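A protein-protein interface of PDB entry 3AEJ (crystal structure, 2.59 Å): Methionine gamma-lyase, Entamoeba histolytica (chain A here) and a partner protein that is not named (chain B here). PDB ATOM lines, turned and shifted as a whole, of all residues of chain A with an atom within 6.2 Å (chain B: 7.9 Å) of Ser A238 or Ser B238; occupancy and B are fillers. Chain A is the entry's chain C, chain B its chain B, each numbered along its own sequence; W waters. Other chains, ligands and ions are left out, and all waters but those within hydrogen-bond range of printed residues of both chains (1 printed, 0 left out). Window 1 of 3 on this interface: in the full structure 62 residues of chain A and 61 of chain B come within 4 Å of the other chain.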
ATOM      1  N   ALA A  79      27.328  -9.807 -18.621  1.00  0.00           N
ATOM      2  CA  ALA A  79      28.247  -8.887 -17.952  1.00  0.00           C
ATOM      3  C   ALA A  79      27.661  -7.479 -17.886  1.00  0.00           C
ATOM      4  O   ALA A  79      26.917  -7.067 -18.778  1.00  0.00           O
ATOM      5  CB  ALA A  79      29.590  -8.873 -18.659  1.00  0.00           C
ATOM      6  N   PHE A  80      28.001  -6.749 -16.828  1.00  0.00           N
ATOM      7  CA  PHE A  80      27.456  -5.412 -16.587  1.00  0.00           C
ATOM      8  C   PHE A  80      28.528  -4.425 -16.145  1.00  0.00           C
ATOM      9  O   PHE A  80      29.639  -4.820 -15.782  1.00  0.00           O
ATOM     10  CB  PHE A  80      26.343  -5.471 -15.536  1.00  0.00           C
ATOM     11  CG  PHE A  80      25.162  -6.296 -15.951  1.00  0.00           C
ATOM     12  CD1 PHE A  80      24.128  -5.728 -16.687  1.00  0.00           C
ATOM     13  CD2 PHE A  80      25.084  -7.642 -15.611  1.00  0.00           C
ATOM     14  CE1 PHE A  80      23.036  -6.490 -17.076  1.00  0.00           C
ATOM     15  CE2 PHE A  80      23.991  -8.411 -15.994  1.00  0.00           C
ATOM     16  CZ  PHE A  80      22.968  -7.834 -16.729  1.00  0.00           C
ATOM     17  N   GLY A  81      28.178  -3.140 -16.175  1.00  0.00           N
ATOM     18  CA  GLY A  81      29.080  -2.062 -15.768  1.00  0.00           C
ATOM     19  C   GLY A  81      29.300  -1.986 -14.268  1.00  0.00           C
ATOM     20  O   GLY A  81      30.269  -1.383 -13.808  1.00  0.00           O
ATOM     21  N   SER A  82      28.393  -2.598 -13.510  1.00  0.00           N
ATOM     22  CA  SER A  82      28.474  -2.636 -12.056  1.00  0.00           C
ATOM     23  C   SER A  82      27.634  -3.789 -11.528  1.00  0.00           C
ATOM     24  O   SER A  82      26.770  -4.311 -12.239  1.00  0.00           O
ATOM     25  CB  SER A  82      27.961  -1.326 -11.463  1.00  0.00           C
ATOM     26  OG  SER A  82      26.571  -1.189 -11.690  1.00  0.00           O
ATOM     27  N   MET A  84      25.442  -3.391  -9.278  1.00  0.00           N
ATOM     28  CA  MET A  84      24.119  -2.777  -9.245  1.00  0.00           C
ATOM     29  C   MET A  84      23.435  -2.831 -10.611  1.00  0.00           C
ATOM     30  O   MET A  84      22.205  -2.843 -10.695  1.00  0.00           O
ATOM     31  CB  MET A  84      24.201  -1.336  -8.734  1.00  0.00           C
ATOM     32  CG  MET A  84      24.580  -1.211  -7.257  1.00  0.00           C
ATOM     33  SD  MET A  84      23.621  -2.247  -6.120  1.00  0.00           S
ATOM     34  CE  MET A  84      21.947  -1.668  -6.407  1.00  0.00           C
ATOM     35  N   GLY A  85      24.240  -2.863 -11.672  1.00  0.00           N
ATOM     36  CA  GLY A  85      23.742  -3.091 -13.024  1.00  0.00           C
ATOM     37  C   GLY A  85      23.172  -4.489 -13.152  1.00  0.00           C
ATOM     38  O   GLY A  85      22.123  -4.685 -13.769  1.00  0.00           O
ATOM     39  N   ALA A  86      23.865  -5.455 -12.552  1.00  0.00           N
ATOM     40  CA  ALA A  86      23.424  -6.848 -12.530  1.00  0.00           C
ATOM     41  C   ALA A  86      22.145  -7.043 -11.713  1.00  0.00           C
ATOM     42  O   ALA A  86      21.247  -7.772 -12.131  1.00  0.00           O
ATOM     43  CB  ALA A  86      24.536  -7.751 -12.004  1.00  0.00           C
ATOM     44  N   SER A  89      19.111  -5.499 -13.481  1.00  0.00           N
ATOM     45  CA  SER A  89      18.770  -6.267 -14.675  1.00  0.00           C
ATOM     46  C   SER A  89      18.370  -7.706 -14.362  1.00  0.00           C
ATOM     47  O   SER A  89      17.947  -8.440 -15.256  1.00  0.00           O
ATOM     48  CB  SER A  89      19.930  -6.260 -15.672  1.00  0.00           C
ATOM     49  OG  SER A  89      20.307  -4.940 -16.026  1.00  0.00           O
ATOM     50  N   ARG A 233      19.184  -5.334 -20.600  1.00  0.00           N
ATOM     51  CA  ARG A 233      20.493  -4.667 -20.617  1.00  0.00           C
ATOM     52  C   ARG A 233      20.674  -3.810 -21.872  1.00  0.00           C
ATOM     53  O   ARG A 233      21.297  -2.746 -21.827  1.00  0.00           O
ATOM     54  CB  ARG A 233      21.622  -5.698 -20.507  1.00  0.00           C
ATOM     55  CG  ARG A 233      23.031  -5.105 -20.441  1.00  0.00           C
ATOM     56  CD  ARG A 233      24.101  -6.188 -20.480  1.00  0.00           C
ATOM     57  NE  ARG A 233      24.211  -6.815 -21.797  1.00  0.00           N
ATOM     58  CZ  ARG A 233      24.911  -7.918 -22.057  1.00  0.00           C
ATOM     59  NH1 ARG A 233      24.941  -8.400 -23.290  1.00  0.00           N
ATOM     60  NH2 ARG A 233      25.575  -8.544 -21.092  1.00  0.00           N
ATOM     61  N   ALA A 236      18.406  -0.750 -20.896  1.00  0.00           N
ATOM     62  CA  ALA A 236      18.849  -0.091 -19.665  1.00  0.00           C
ATOM     63  C   ALA A 236      20.270   0.452 -19.794  1.00  0.00           C
ATOM     64  O   ALA A 236      20.565   1.546 -19.316  1.00  0.00           O
ATOM     65  CB  ALA A 236      18.741  -1.026 -18.489  1.00  0.00           C
ATOM     66  N   GLY A 237      21.146  -0.327 -20.423  1.00  0.00           N
ATOM     67  CA  GLY A 237      22.452   0.164 -20.857  1.00  0.00           C
ATOM     68  C   GLY A 237      23.636   0.038 -19.917  1.00  0.00           C
ATOM     69  O   GLY A 237      24.627   0.749 -20.088  1.00  0.00           O
ATOM     70  N   SER A 238      23.549  -0.857 -18.935  1.00  0.00           N
ATOM     71  CA  SER A 238      24.676  -1.112 -18.037  1.00  0.00           C
ATOM     72  C   SER A 238      25.606  -2.162 -18.633  1.00  0.00           C
ATOM     73  O   SER A 238      25.341  -3.361 -18.551  1.00  0.00           O
ATOM     74  CB  SER A 238      24.201  -1.533 -16.648  1.00  0.00           C
ATOM     75  OG  SER A 238      25.307  -1.807 -15.804  1.00  0.00           O
ATOM     76  N   LEU A 239      26.699  -1.698 -19.227  1.00  0.00           N
ATOM     77  CA  LEU A 239      27.594  -2.567 -19.983  1.00  0.00           C
ATOM     78  C   LEU A 239      28.995  -2.635 -19.393  1.00  0.00           C
ATOM     79  O   LEU A 239      29.525  -1.636 -18.906  1.00  0.00           O
ATOM     80  CB  LEU A 239      27.686  -2.095 -21.438  1.00  0.00           C
ATOM     81  CG  LEU A 239      26.402  -1.815 -22.226  1.00  0.00           C
ATOM     82  CD1 LEU A 239      26.742  -1.110 -23.529  1.00  0.00           C
ATOM     83  CD2 LEU A 239      25.604  -3.095 -22.487  1.00  0.00           C
ATOM     84  N   MET A 240      29.590  -3.822 -19.448  1.00  0.00           N
ATOM     85  CA  MET A 240      31.001  -3.989 -19.129  1.00  0.00           C
ATOM     86  C   MET A 240      31.830  -3.524 -20.323  1.00  0.00           C
ATOM     87  O   MET A 240      31.574  -3.924 -21.461  1.00  0.00           O
ATOM     88  CB  MET A 240      31.311  -5.450 -18.786  1.00  0.00           C
ATOM     89  CG  MET A 240      32.747  -5.712 -18.344  1.00  0.00           C
ATOM     90  SD  MET A 240      32.995  -7.371 -17.674  1.00  0.00           S
ATOM     91  CE  MET A 240      32.321  -7.188 -16.024  1.00  0.00           C
ATOM     92  N   ARG B  55      31.775   4.045  -8.626  1.00  0.00           N
ATOM     93  CA  ARG B  55      30.361   4.145  -9.002  1.00  0.00           C
ATOM     94  C   ARG B  55      29.746   5.462  -8.528  1.00  0.00           C
ATOM     95  O   ARG B  55      28.968   6.089  -9.251  1.00  0.00           O
ATOM     96  CB  ARG B  55      29.562   2.953  -8.463  1.00  0.00           C
ATOM     97  CG  ARG B  55      28.063   3.021  -8.750  1.00  0.00           C
ATOM     98  CD  ARG B  55      27.398   1.646  -8.739  1.00  0.00           C
ATOM     99  NE  ARG B  55      27.812   0.824  -7.604  1.00  0.00           N
ATOM    100  CZ  ARG B  55      27.323   0.922  -6.371  1.00  0.00           C
ATOM    101  NH1 ARG B  55      26.382   1.814  -6.080  1.00  0.00           N
ATOM    102  NH2 ARG B  55      27.780   0.118  -5.424  1.00  0.00           N
ATOM    103  N   ALA B  78      26.359  13.782 -16.192  1.00  0.00           N
ATOM    104  CA  ALA B  78      26.609  12.422 -15.730  1.00  0.00           C
ATOM    105  C   ALA B  78      26.962  11.519 -16.906  1.00  0.00           C
ATOM    106  O   ALA B  78      26.260  11.509 -17.917  1.00  0.00           O
ATOM    107  CB  ALA B  78      25.396  11.885 -14.986  1.00  0.00           C
ATOM    108  N   ALA B  79      28.054  10.769 -16.768  1.00  0.00           N
ATOM    109  CA  ALA B  79      28.505   9.848 -17.813  1.00  0.00           C
ATOM    110  C   ALA B  79      27.991   8.430 -17.577  1.00  0.00           C
ATOM    111  O   ALA B  79      27.823   8.000 -16.434  1.00  0.00           O
ATOM    112  CB  ALA B  79      30.021   9.859 -17.916  1.00  0.00           C
ATOM    113  N   PHE B  80      27.744   7.712 -18.670  1.00  0.00           N
ATOM    114  CA  PHE B  80      27.153   6.378 -18.614  1.00  0.00           C
ATOM    115  C   PHE B  80      27.885   5.406 -19.537  1.00  0.00           C
ATOM    116  O   PHE B  80      28.646   5.824 -20.413  1.00  0.00           O
ATOM    117  CB  PHE B  80      25.669   6.439 -18.993  1.00  0.00           C
ATOM    118  CG  PHE B  80      24.838   7.281 -18.065  1.00  0.00           C
ATOM    119  CD1 PHE B  80      24.237   6.716 -16.946  1.00  0.00           C
ATOM    120  CD2 PHE B  80      24.650   8.638 -18.310  1.00  0.00           C
ATOM    121  CE1 PHE B  80      23.466   7.490 -16.085  1.00  0.00           C
ATOM    122  CE2 PHE B  80      23.879   9.418 -17.456  1.00  0.00           C
ATOM    123  CZ  PHE B  80      23.286   8.842 -16.341  1.00  0.00           C
ATOM    124  N   GLY B  81      27.643   4.111 -19.337  1.00  0.00           N
ATOM    125  CA  GLY B  81      28.253   3.061 -20.155  1.00  0.00           C
ATOM    126  C   GLY B  81      27.665   2.929 -21.548  1.00  0.00           C
ATOM    127  O   GLY B  81      28.172   2.166 -22.372  1.00  0.00           O
ATOM    128  N   SER B  82      26.591   3.673 -21.805  1.00  0.00           N
ATOM    129  CA  SER B  82      25.925   3.686 -23.105  1.00  0.00           C
ATOM    130  C   SER B  82      24.972   4.868 -23.181  1.00  0.00           C
ATOM    131  O   SER B  82      24.532   5.385 -22.151  1.00  0.00           O
ATOM    132  CB  SER B  82      25.146   2.387 -23.330  1.00  0.00           C
ATOM    133  OG  SER B  82      24.163   2.213 -22.326  1.00  0.00           O
ATOM    134  N   GLY B  83      24.659   5.290 -24.404  1.00  0.00           N
ATOM    135  CA  GLY B  83      23.632   6.301 -24.644  1.00  0.00           C
ATOM    136  C   GLY B  83      22.292   5.856 -24.086  1.00  0.00           C
ATOM    137  O   GLY B  83      21.518   6.674 -23.585  1.00  0.00           O
ATOM    138  N   MET B  84      22.028   4.551 -24.166  1.00  0.00           N
ATOM    139  CA  MET B  84      20.823   3.957 -23.592  1.00  0.00           C
ATOM    140  C   MET B  84      20.800   4.086 -22.071  1.00  0.00           C
ATOM    141  O   MET B  84      19.735   4.275 -21.474  1.00  0.00           O
ATOM    142  CB  MET B  84      20.683   2.488 -24.003  1.00  0.00           C
ATOM    143  CG  MET B  84      20.370   2.267 -25.479  1.00  0.00           C
ATOM    144  SD  MET B  84      19.046   3.312 -26.124  1.00  0.00           S
ATOM    145  CE  MET B  84      17.636   2.787 -25.141  1.00  0.00           C
ATOM    146  N   GLY B  85      21.977   3.982 -21.456  1.00  0.00           N
ATOM    147  CA  GLY B  85      22.132   4.224 -20.023  1.00  0.00           C
ATOM    148  C   GLY B  85      21.734   5.644 -19.670  1.00  0.00           C
ATOM    149  O   GLY B  85      21.072   5.880 -18.655  1.00  0.00           O
ATOM    150  N   ALA B  86      22.130   6.585 -20.525  1.00  0.00           N
ATOM    151  CA  ALA B  86      21.780   7.990 -20.361  1.00  0.00           C
ATOM    152  C   ALA B  86      20.280   8.210 -20.520  1.00  0.00           C
ATOM    153  O   ALA B  86      19.676   8.944 -19.740  1.00  0.00           O
ATOM    154  CB  ALA B  86      22.559   8.855 -21.347  1.00  0.00           C
ATOM    155  N   ILE B  87      19.688   7.562 -21.522  1.00  0.00           N
ATOM    156  CA  ILE B  87      18.259   7.709 -21.818  1.00  0.00           C
ATOM    157  C   ILE B  87      17.384   7.135 -20.696  1.00  0.00           C
ATOM    158  O   ILE B  87      16.454   7.799 -20.234  1.00  0.00           O
ATOM    159  CB  ILE B  87      17.896   7.096 -23.199  1.00  0.00           C
ATOM    160  CG1 ILE B  87      18.617   7.860 -24.316  1.00  0.00           C
ATOM    161  CG2 ILE B  87      16.385   7.118 -23.427  1.00  0.00           C
ATOM    162  CD1 ILE B  87      18.685   7.136 -25.652  1.00  0.00           C
ATOM    163  N   SER B  88      17.699   5.915 -20.260  1.00  0.00           N
ATOM    164  CA  SER B  88      16.982   5.259 -19.162  1.00  0.00           C
ATOM    165  C   SER B  88      17.053   6.070 -17.871  1.00  0.00           C
ATOM    166  O   SER B  88      16.046   6.246 -17.186  1.00  0.00           O
ATOM    167  CB  SER B  88      17.538   3.858 -18.920  1.00  0.00           C
ATOM    168  OG  SER B  88      17.360   3.041 -20.061  1.00  0.00           O
ATOM    169  N   SER B  89      18.247   6.571 -17.559  1.00  0.00           N
ATOM    170  CA  SER B  89      18.473   7.354 -16.349  1.00  0.00           C
ATOM    171  C   SER B  89      17.880   8.759 -16.412  1.00  0.00           C
ATOM    172  O   SER B  89      17.578   9.350 -15.377  1.00  0.00           O
ATOM    173  CB  SER B  89      19.965   7.429 -16.033  1.00  0.00           C
ATOM    174  OG  SER B  89      20.521   6.132 -15.903  1.00  0.00           O
ATOM    175  N   GLY B 215      29.314   4.764 -24.965  1.00  0.00           N
ATOM    176  CA  GLY B 215      29.096   5.640 -23.818  1.00  0.00           C
ATOM    177  C   GLY B 215      27.921   6.584 -23.968  1.00  0.00           C
ATOM    178  O   GLY B 215      27.428   6.816 -25.073  1.00  0.00           O
ATOM    179  N   GLY B 216      27.473   7.125 -22.840  1.00  0.00           N
ATOM    180  CA  GLY B 216      26.400   8.113 -22.819  1.00  0.00           C
ATOM    181  C   GLY B 216      26.688   9.227 -21.834  1.00  0.00           C
ATOM    182  O   GLY B 216      27.471   9.057 -20.898  1.00  0.00           O
ATOM    183  N   TYR B 232      20.049   7.935  -9.447  1.00  0.00           N
ATOM    184  CA  TYR B 232      19.522   6.803 -10.214  1.00  0.00           C
ATOM    185  C   TYR B 232      20.651   5.919 -10.754  1.00  0.00           C
ATOM    186  O   TYR B 232      20.574   4.697 -10.662  1.00  0.00           O
ATOM    187  CB  TYR B 232      18.615   7.281 -11.354  1.00  0.00           C
ATOM    188  CG  TYR B 232      17.920   6.167 -12.115  1.00  0.00           C
ATOM    189  CD1 TYR B 232      18.479   5.635 -13.277  1.00  0.00           C
ATOM    190  CD2 TYR B 232      16.703   5.645 -11.673  1.00  0.00           C
ATOM    191  CE1 TYR B 232      17.846   4.616 -13.984  1.00  0.00           C
ATOM    192  CE2 TYR B 232      16.063   4.620 -12.374  1.00  0.00           C
ATOM    193  CZ  TYR B 232      16.643   4.112 -13.526  1.00  0.00           C
ATOM    194  OH  TYR B 232      16.021   3.100 -14.224  1.00  0.00           O
ATOM    195  N   ARG B 233      21.690   6.546 -11.307  1.00  0.00           N
ATOM    196  CA  ARG B 233      22.867   5.831 -11.818  1.00  0.00           C
ATOM    197  C   ARG B 233      23.551   5.011 -10.717  1.00  0.00           C
ATOM    198  O   ARG B 233      24.093   3.937 -10.980  1.00  0.00           O
ATOM    199  CB  ARG B 233      23.861   6.811 -12.459  1.00  0.00           C
ATOM    200  CG  ARG B 233      25.095   6.151 -13.084  1.00  0.00           C
ATOM    201  CD  ARG B 233      26.102   7.171 -13.594  1.00  0.00           C
ATOM    202  NE  ARG B 233      26.669   7.982 -12.516  1.00  0.00           N
ATOM    203  CZ  ARG B 233      27.584   8.936 -12.683  1.00  0.00           C
ATOM    204  NH1 ARG B 233      28.025   9.611 -11.632  1.00  0.00           N
ATOM    205  NH2 ARG B 233      28.059   9.217 -13.891  1.00  0.00           N
ATOM    206  N   LYS B 234      23.507   5.529  -9.491  1.00  0.00           N
ATOM    207  CA  LYS B 234      24.036   4.849  -8.309  1.00  0.00           C
ATOM    208  C   LYS B 234      23.415   3.458  -8.107  1.00  0.00           C
ATOM    209  O   LYS B 234      24.112   2.513  -7.729  1.00  0.00           O
ATOM    210  CB  LYS B 234      23.814   5.722  -7.067  1.00  0.00           C
ATOM    211  CG  LYS B 234      24.358   5.147  -5.761  1.00  0.00           C
ATOM    212  CD  LYS B 234      23.970   6.014  -4.561  1.00  0.00           C
ATOM    213  CE  LYS B 234      22.596   5.654  -4.006  1.00  0.00           C
ATOM    214  NZ  LYS B 234      22.597   4.345  -3.292  1.00  0.00           N
ATOM    215  N   ASP B 235      22.112   3.343  -8.363  1.00  0.00           N
ATOM    216  CA  ASP B 235      21.383   2.088  -8.164  1.00  0.00           C
ATOM    217  C   ASP B 235      21.171   1.297  -9.456  1.00  0.00           C
ATOM    218  O   ASP B 235      21.168   0.063  -9.438  1.00  0.00           O
ATOM    219  CB  ASP B 235      20.038   2.345  -7.472  1.00  0.00           C
ATOM    220  CG  ASP B 235      20.194   2.897  -6.058  1.00  0.00           C
ATOM    221  OD1 ASP B 235      19.245   3.548  -5.574  1.00  0.00           O
ATOM    222  OD2 ASP B 235      21.254   2.687  -5.428  1.00  0.00           O
ATOM    223  N   ALA B 236      20.992   2.005 -10.571  1.00  0.00           N
ATOM    224  CA  ALA B 236      20.818   1.365 -11.875  1.00  0.00           C
ATOM    225  C   ALA B 236      22.122   0.743 -12.372  1.00  0.00           C
ATOM    226  O   ALA B 236      22.123  -0.377 -12.881  1.00  0.00           O
ATOM    227  CB  ALA B 236      20.272   2.349 -12.890  1.00  0.00           C
ATOM    228  N   GLY B 237      23.220   1.483 -12.233  1.00  0.00           N
ATOM    229  CA  GLY B 237      24.557   0.936 -12.449  1.00  0.00           C
ATOM    230  C   GLY B 237      25.135   0.969 -13.853  1.00  0.00           C
ATOM    231  O   GLY B 237      26.029   0.182 -14.169  1.00  0.00           O
ATOM    232  N   SER B 238      24.636   1.872 -14.696  1.00  0.00           N
ATOM    233  CA  SER B 238      25.223   2.089 -16.017  1.00  0.00           C
ATOM    234  C   SER B 238      26.352   3.111 -15.921  1.00  0.00           C
ATOM    235  O   SER B 238      26.120   4.321 -15.939  1.00  0.00           O
ATOM    236  CB  SER B 238      24.166   2.533 -17.029  1.00  0.00           C
ATOM    237  OG  SER B 238      24.747   2.756 -18.300  1.00  0.00           O
ATOM    238  N   LEU B 239      27.575   2.607 -15.810  1.00  0.00           N
ATOM    239  CA  LEU B 239      28.739   3.454 -15.576  1.00  0.00           C
ATOM    240  C   LEU B 239      29.671   3.485 -16.774  1.00  0.00           C
ATOM    241  O   LEU B 239      29.760   2.514 -17.529  1.00  0.00           O
ATOM    242  CB  LEU B 239      29.520   2.967 -14.351  1.00  0.00           C
ATOM    243  CG  LEU B 239      28.785   2.776 -13.023  1.00  0.00           C
ATOM    244  CD1 LEU B 239      29.676   2.021 -12.059  1.00  0.00           C
ATOM    245  CD2 LEU B 239      28.339   4.107 -12.424  1.00  0.00           C
ATOM    246  N   MET B 240      30.364   4.607 -16.939  1.00  0.00           N
ATOM    247  CA  MET B 240      31.443   4.706 -17.907  1.00  0.00           C
ATOM    248  C   MET B 240      32.725   4.205 -17.254  1.00  0.00           C
ATOM    249  O   MET B 240      33.094   4.656 -16.167  1.00  0.00           O
ATOM    250  CB  MET B 240      31.607   6.150 -18.390  1.00  0.00           C
ATOM    251  CG  MET B 240      32.678   6.337 -19.460  1.00  0.00           C
ATOM    252  SD  MET B 240      32.689   8.001 -20.149  1.00  0.00           S
ATOM    253  CE  MET B 240      31.379   7.898 -21.364  1.00  0.00           C
ATOM    254  N   ALA B 241      33.386   3.257 -17.913  1.00  0.00           N
ATOM    255  CA  ALA B 241      34.665   2.732 -17.445  1.00  0.00           C
ATOM    256  C   ALA B 241      35.740   3.818 -17.466  1.00  0.00           C
ATOM    257  O   ALA B 241      35.735   4.668 -18.360  1.00  0.00           O
ATOM    258  CB  ALA B 241      35.093   1.555 -18.298  1.00  0.00           C
HETATM  259  O   HOH W   1      27.880   0.483 -17.944  1.00  0.00           O
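O of Gly A85 is in hydrogen-bond range of OG of Ser A89, at 2.9 Å. The backbone NH (N) of Gly B216 lies close to the backbone carbonyl oxygen (O) of Ser B82 (3.5 Å). The backbone NH (N) of Gly A81 sits at hydrogen-bond distance from the side-chain hydroxyl (OG) of Ser A238 (3.2 Å). The backbone NH (N) of Gly B81 lies close to the backbone carbonyl oxygen (O) of Leu B239 (3.2 Å). OG of Ser A82 lies close to N of Met A84. NH1 of Arg B55 is in hydrogen-bond range of O of Lys B234 (2.9 Å).
Among the printed residues, merely in contact across the chains: Ala A236 with Gly B85, Ala A236 with Ser B88, Ala A236 with Met B84, Met A84 with Arg B55, Leu A239 with Gly B81, Met A84 with Lys B234, Ser A82 with Leu B239, Ser A238 with Ser B238, Leu A239 with Ser B82, Gly A81 with Leu B239, Gly A85 with Gly B237, Gly A237 with Gly B85 and Gly A81 with Gly B237.
Of the printed residues of chain B, Gly A85 touches Ala B236 and Gly B237. Of the printed residues of chain B, Gly A237 touches Ser B82 (2.7 Å), Gly B85 (3.9 Å) and Ser B238 (2.7 Å). Ser A238 touches two residues of chain B. Printed residues of chain A within 4 Å of Arg B55: Met A84 (3.6 Å). Ala B79 touches none of the printed residues of chain A. Ser B238 touches just these residues of chain A: Gly A237 and Ser A238. The nearest residue of chain A that does not touch Ser B238 is Ala A236 (4.4 Å). The nearest printed residue of chain A that does not touch Ala B236 is Ser A238 (4.5 Å).
Water W1 bridges the backbone NH (N) of Leu A239 and the backbone carbonyl oxygen (O) of Leu B239.
The backbone carbonyl oxygen of Ala B236 lies close to the backbone carbonyl oxygen of Met A84 (3.3 Å). The backbone carbonyl oxygen of Gly B237 sits at hydrogen-bond distance from the side-chain hydroxyl of Ser A82. O of Ala B236 sits close to N of Gly A85 (3.5 Å). The backbone carbonyl oxygen (O) of Asp B235 lies close to the backbone carbonyl oxygen (O) of Met A84, at 3.3 Å. O of Gly A237 lies within hydrogen-bond range of OG of Ser B82 (2.7 Å). The backbone carbonyl oxygen (O) of Gly B237 is in hydrogen-bond range of the side-chain hydroxyl (OG) of Ser A238 (2.7 Å). OG of Ser B238 lies within hydrogen-bond range of O of Gly A237 (2.7 Å).
Of the 14 printed residues of chain A, 8 touch a printed residue of chain B. Hydrophobic or aromatic side chains of chain A within 4 Å of the printed part of chain B: Met A84 and Leu A239. Hydrophobic or aromatic side chains of chain B that line the printed part of chain A: Leu B239.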
